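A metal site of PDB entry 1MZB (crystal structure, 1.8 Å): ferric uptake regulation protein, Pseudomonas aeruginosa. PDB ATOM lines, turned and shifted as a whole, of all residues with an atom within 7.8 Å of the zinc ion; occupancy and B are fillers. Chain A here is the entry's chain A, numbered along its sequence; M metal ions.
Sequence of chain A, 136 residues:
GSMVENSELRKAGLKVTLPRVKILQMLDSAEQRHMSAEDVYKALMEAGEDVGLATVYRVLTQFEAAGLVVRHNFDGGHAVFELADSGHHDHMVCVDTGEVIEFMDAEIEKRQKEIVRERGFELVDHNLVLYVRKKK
OE2 of Glu 82 lies within hydrogen-bond range of ND1 of His 72, at 2.8 Å.
Four residues have an atom within 4 Å of the zinc ion: His 34, Glu 82, His 91 and Glu 102.
The nearest printed residue that does not touch the zinc ion is His 89 (5.0 Å).
The zinc ion is bound by NE2 of His 34 (2.0 Å), OE1 of Glu 82 (2.0 Å), NE2 of His 91 (2.0 Å) and OE2 of Glu 102 (2.2 Å).
Slightly farther from the zinc ion lies OE2 of Glu 82 (2.8 Å).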
ATOM      1  N   ARG A  33      17.499 -19.096 -17.048  1.00  0.00           N
ATOM      2  CA  ARG A  33      18.259 -18.058 -17.723  1.00  0.00           C
ATOM      3  C   ARG A  33      17.325 -16.989 -18.308  1.00  0.00           C
ATOM      4  O   ARG A  33      17.678 -15.787 -18.357  1.00  0.00           O
ATOM      5  CB  ARG A  33      19.110 -18.676 -18.840  1.00  0.00           C
ATOM      6  CG  ARG A  33      19.792 -19.995 -18.467  1.00  0.00           C
ATOM      7  CD  ARG A  33      20.919 -20.309 -19.454  1.00  0.00           C
ATOM      8  NE  ARG A  33      21.474 -21.648 -19.270  1.00  0.00           N
ATOM      9  CZ  ARG A  33      22.577 -22.074 -19.880  1.00  0.00           C
ATOM     10  NH1 ARG A  33      23.231 -21.266 -20.712  1.00  0.00           N
ATOM     11  NH2 ARG A  33      23.025 -23.319 -19.671  1.00  0.00           N
ATOM     12  N   HIS A  34      16.135 -17.434 -18.718  1.00  0.00           N
ATOM     13  CA  HIS A  34      15.118 -16.570 -19.330  1.00  0.00           C
ATOM     14  C   HIS A  34      13.823 -16.527 -18.520  1.00  0.00           C
ATOM     15  O   HIS A  34      12.852 -17.234 -18.790  1.00  0.00           O
ATOM     16  CB  HIS A  34      14.829 -17.040 -20.747  1.00  0.00           C
ATOM     17  CG  HIS A  34      16.063 -17.231 -21.563  1.00  0.00           C
ATOM     18  ND1 HIS A  34      16.678 -18.459 -21.672  1.00  0.00           N
ATOM     19  CD2 HIS A  34      16.805 -16.303 -22.215  1.00  0.00           C
ATOM     20  CE1 HIS A  34      17.781 -18.256 -22.367  1.00  0.00           C
ATOM     21  NE2 HIS A  34      17.908 -16.963 -22.729  1.00  0.00           N
ATOM     22  N   HIS A  72      12.507 -10.254 -24.535  1.00  0.00           N
ATOM     23  CA  HIS A  72      12.336 -11.107 -25.691  1.00  0.00           C
ATOM     24  C   HIS A  72      10.957 -11.793 -25.563  1.00  0.00           C
ATOM     25  O   HIS A  72      10.439 -11.910 -24.466  1.00  0.00           O
ATOM     26  CB  HIS A  72      13.362 -12.253 -25.686  1.00  0.00           C
ATOM     27  CG  HIS A  72      14.751 -11.843 -26.081  1.00  0.00           C
ATOM     28  ND1 HIS A  72      15.812 -11.896 -25.194  1.00  0.00           N
ATOM     29  CD2 HIS A  72      15.275 -11.526 -27.282  1.00  0.00           C
ATOM     30  CE1 HIS A  72      16.933 -11.625 -25.842  1.00  0.00           C
ATOM     31  NE2 HIS A  72      16.638 -11.407 -27.115  1.00  0.00           N
ATOM     32  N   PHE A  74       9.731 -15.224 -26.996  1.00  0.00           N
ATOM     33  CA  PHE A  74      10.074 -16.383 -27.827  1.00  0.00           C
ATOM     34  C   PHE A  74       8.928 -17.305 -28.217  1.00  0.00           C
ATOM     35  O   PHE A  74       8.978 -17.908 -29.305  1.00  0.00           O
ATOM     36  CB  PHE A  74      11.133 -17.241 -27.122  1.00  0.00           C
ATOM     37  CG  PHE A  74      12.434 -16.508 -26.843  1.00  0.00           C
ATOM     38  CD1 PHE A  74      13.176 -15.950 -27.885  1.00  0.00           C
ATOM     39  CD2 PHE A  74      12.943 -16.464 -25.540  1.00  0.00           C
ATOM     40  CE1 PHE A  74      14.453 -15.369 -27.630  1.00  0.00           C
ATOM     41  CE2 PHE A  74      14.190 -15.872 -25.280  1.00  0.00           C
ATOM     42  CZ  PHE A  74      14.942 -15.328 -26.319  1.00  0.00           C
ATOM     43  N   VAL A  80      10.139 -12.543 -21.814  1.00  0.00           N
ATOM     44  CA  VAL A  80      11.233 -13.071 -21.037  1.00  0.00           C
ATOM     45  C   VAL A  80      12.171 -11.892 -20.805  1.00  0.00           C
ATOM     46  O   VAL A  80      12.363 -11.114 -21.728  1.00  0.00           O
ATOM     47  CB  VAL A  80      11.988 -14.128 -21.853  1.00  0.00           C
ATOM     48  CG1 VAL A  80      13.426 -14.257 -21.404  1.00  0.00           C
ATOM     49  CG2 VAL A  80      11.240 -15.458 -21.708  1.00  0.00           C
ATOM     50  N   PHE A  81      12.767 -11.776 -19.613  1.00  0.00           N
ATOM     51  CA  PHE A  81      13.676 -10.661 -19.367  1.00  0.00           C
ATOM     52  C   PHE A  81      15.007 -11.273 -18.970  1.00  0.00           C
ATOM     53  O   PHE A  81      15.033 -12.178 -18.154  1.00  0.00           O
ATOM     54  CB  PHE A  81      13.175  -9.800 -18.202  1.00  0.00           C
ATOM     55  CG  PHE A  81      11.885  -9.073 -18.498  1.00  0.00           C
ATOM     56  CD1 PHE A  81      10.650  -9.683 -18.292  1.00  0.00           C
ATOM     57  CD2 PHE A  81      11.908  -7.754 -18.974  1.00  0.00           C
ATOM     58  CE1 PHE A  81       9.427  -8.970 -18.545  1.00  0.00           C
ATOM     59  CE2 PHE A  81      10.714  -7.051 -19.231  1.00  0.00           C
ATOM     60  CZ  PHE A  81       9.468  -7.657 -19.008  1.00  0.00           C
ATOM     61  N   GLU A  82      16.099 -10.830 -19.573  1.00  0.00           N
ATOM     62  CA  GLU A  82      17.402 -11.400 -19.212  1.00  0.00           C
ATOM     63  C   GLU A  82      18.403 -10.270 -19.178  1.00  0.00           C
ATOM     64  O   GLU A  82      18.199  -9.253 -19.807  1.00  0.00           O
ATOM     65  CB  GLU A  82      17.834 -12.478 -20.198  1.00  0.00           C
ATOM     66  CG  GLU A  82      17.885 -12.041 -21.675  1.00  0.00           C
ATOM     67  CD  GLU A  82      18.107 -13.221 -22.642  1.00  0.00           C
ATOM     68  OE1 GLU A  82      19.198 -13.814 -22.642  1.00  0.00           O
ATOM     69  OE2 GLU A  82      17.179 -13.547 -23.399  1.00  0.00           O
ATOM     70  N   LEU A  83      19.451 -10.427 -18.393  1.00  0.00           N
ATOM     71  CA  LEU A  83      20.445  -9.380 -18.336  1.00  0.00           C
ATOM     72  C   LEU A  83      21.058  -9.121 -19.704  1.00  0.00           C
ATOM     73  O   LEU A  83      21.114 -10.012 -20.585  1.00  0.00           O
ATOM     74  CB  LEU A  83      21.529  -9.782 -17.340  1.00  0.00           C
ATOM     75  CG  LEU A  83      21.020  -9.908 -15.922  1.00  0.00           C
ATOM     76  CD1 LEU A  83      22.142 -10.520 -15.059  1.00  0.00           C
ATOM     77  CD2 LEU A  83      20.595  -8.509 -15.380  1.00  0.00           C
ATOM     78  N   SER A  86      25.547  -9.752 -19.515  1.00  0.00           N
ATOM     79  CA  SER A  86      26.115 -11.072 -19.752  1.00  0.00           C
ATOM     80  C   SER A  86      26.723 -11.153 -21.153  1.00  0.00           C
ATOM     81  O   SER A  86      26.411 -10.334 -22.033  1.00  0.00           O
ATOM     82  CB  SER A  86      25.034 -12.147 -19.601  1.00  0.00           C
ATOM     83  OG  SER A  86      24.000 -11.966 -20.570  1.00  0.00           O
ATOM     84  N   GLY A  87      27.591 -12.147 -21.382  1.00  0.00           N
ATOM     85  CA  GLY A  87      28.181 -12.307 -22.697  1.00  0.00           C
ATOM     86  C   GLY A  87      27.040 -12.321 -23.702  1.00  0.00           C
ATOM     87  O   GLY A  87      25.913 -12.692 -23.363  1.00  0.00           O
ATOM     88  N   HIS A  88      27.315 -11.911 -24.933  1.00  0.00           N
ATOM     89  CA  HIS A  88      26.274 -11.889 -25.959  1.00  0.00           C
ATOM     90  C   HIS A  88      25.825 -13.297 -26.326  1.00  0.00           C
ATOM     91  O   HIS A  88      26.615 -14.257 -26.307  1.00  0.00           O
ATOM     92  CB  HIS A  88      26.772 -11.190 -27.229  1.00  0.00           C
ATOM     93  CG  HIS A  88      25.886 -11.378 -28.436  1.00  0.00           C
ATOM     94  ND1 HIS A  88      24.660 -10.769 -28.558  1.00  0.00           N
ATOM     95  CD2 HIS A  88      26.090 -12.063 -29.581  1.00  0.00           C
ATOM     96  CE1 HIS A  88      24.148 -11.055 -29.742  1.00  0.00           C
ATOM     97  NE2 HIS A  88      25.002 -11.848 -30.393  1.00  0.00           N
ATOM     98  N   HIS A  89      24.543 -13.407 -26.656  1.00  0.00           N
ATOM     99  CA  HIS A  89      23.946 -14.674 -27.039  1.00  0.00           C
ATOM    100  C   HIS A  89      22.719 -14.429 -27.901  1.00  0.00           C
ATOM    101  O   HIS A  89      21.938 -13.511 -27.660  1.00  0.00           O
ATOM    102  CB  HIS A  89      23.571 -15.473 -25.780  1.00  0.00           C
ATOM    103  N   ASP A  90      22.581 -15.229 -28.951  1.00  0.00           N
ATOM    104  CA  ASP A  90      21.412 -15.134 -29.800  1.00  0.00           C
ATOM    105  C   ASP A  90      20.663 -16.383 -29.369  1.00  0.00           C
ATOM    106  O   ASP A  90      21.102 -17.046 -28.458  1.00  0.00           O
ATOM    107  CB  ASP A  90      21.821 -15.184 -31.232  1.00  0.00           C
ATOM    108  CG  ASP A  90      22.740 -13.997 -31.577  1.00  0.00           C
ATOM    109  OD1 ASP A  90      22.364 -12.856 -31.286  1.00  0.00           O
ATOM    110  OD2 ASP A  90      23.771 -14.235 -32.120  1.00  0.00           O
ATOM    111  N   HIS A  91      19.555 -16.724 -30.006  1.00  0.00           N
ATOM    112  CA  HIS A  91      18.793 -17.861 -29.482  1.00  0.00           C
ATOM    113  C   HIS A  91      18.197 -18.786 -30.507  1.00  0.00           C
ATOM    114  O   HIS A  91      17.762 -18.330 -31.568  1.00  0.00           O
ATOM    115  CB  HIS A  91      17.602 -17.343 -28.619  1.00  0.00           C
ATOM    116  CG  HIS A  91      17.987 -16.453 -27.473  1.00  0.00           C
ATOM    117  ND1 HIS A  91      18.303 -15.122 -27.652  1.00  0.00           N
ATOM    118  CD2 HIS A  91      18.124 -16.772 -26.172  1.00  0.00           C
ATOM    119  CE1 HIS A  91      18.626 -14.679 -26.460  1.00  0.00           C
ATOM    120  NE2 HIS A  91      18.542 -15.625 -25.551  1.00  0.00           N
ATOM    121  N   VAL A 100      14.355 -22.868 -25.110  1.00  0.00           N
ATOM    122  CA  VAL A 100      15.240 -21.821 -25.655  1.00  0.00           C
ATOM    123  C   VAL A 100      16.670 -22.239 -25.432  1.00  0.00           C
ATOM    124  O   VAL A 100      17.071 -22.585 -24.289  1.00  0.00           O
ATOM    125  CB  VAL A 100      14.990 -20.486 -24.952  1.00  0.00           C
ATOM    126  CG1 VAL A 100      15.948 -19.413 -25.471  1.00  0.00           C
ATOM    127  CG2 VAL A 100      13.514 -20.062 -25.196  1.00  0.00           C
ATOM    128  N   ILE A 101      17.445 -22.176 -26.507  1.00  0.00           N
ATOM    129  CA  ILE A 101      18.855 -22.568 -26.508  1.00  0.00           C
ATOM    130  C   ILE A 101      19.693 -21.363 -26.945  1.00  0.00           C
ATOM    131  O   ILE A 101      19.553 -20.859 -28.055  1.00  0.00           O
ATOM    132  CB  ILE A 101      19.071 -23.736 -27.515  1.00  0.00           C
ATOM    133  CG1 ILE A 101      18.225 -24.938 -27.096  1.00  0.00           C
ATOM    134  CG2 ILE A 101      20.571 -24.089 -27.621  1.00  0.00           C
ATOM    135  CD1 ILE A 101      18.059 -25.974 -28.184  1.00  0.00           C
ATOM    136  N   GLU A 102      20.562 -20.885 -26.053  1.00  0.00           N
ATOM    137  CA  GLU A 102      21.439 -19.768 -26.423  1.00  0.00           C
ATOM    138  C   GLU A 102      22.626 -20.262 -27.268  1.00  0.00           C
ATOM    139  O   GLU A 102      23.107 -21.403 -27.114  1.00  0.00           O
ATOM    140  CB  GLU A 102      22.009 -19.064 -25.186  1.00  0.00           C
ATOM    141  CG  GLU A 102      21.001 -18.233 -24.407  1.00  0.00           C
ATOM    142  CD  GLU A 102      21.658 -17.351 -23.351  1.00  0.00           C
ATOM    143  OE1 GLU A 102      22.764 -17.717 -22.879  1.00  0.00           O
ATOM    144  OE2 GLU A 102      21.062 -16.318 -22.969  1.00  0.00           O
ATOM    145  N   PHE A 103      23.100 -19.409 -28.172  1.00  0.00           N
ATOM    146  CA  PHE A 103      24.281 -19.729 -28.972  1.00  0.00           C
ATOM    147  C   PHE A 103      24.943 -18.424 -29.339  1.00  0.00           C
ATOM    148  O   PHE A 103      24.346 -17.352 -29.220  1.00  0.00           O
ATOM    149  CB  PHE A 103      23.930 -20.537 -30.224  1.00  0.00           C
ATOM    150  CG  PHE A 103      23.241 -19.740 -31.304  1.00  0.00           C
ATOM    151  CD1 PHE A 103      21.860 -19.561 -31.298  1.00  0.00           C
ATOM    152  CD2 PHE A 103      23.984 -19.182 -32.324  1.00  0.00           C
ATOM    153  CE1 PHE A 103      21.218 -18.834 -32.312  1.00  0.00           C
ATOM    154  CE2 PHE A 103      23.374 -18.446 -33.353  1.00  0.00           C
ATOM    155  CZ  PHE A 103      21.981 -18.273 -33.342  1.00  0.00           C
HETATM  156 ZN    ZN M   1      19.119 -15.617 -23.588  1.00  0.00          ZN
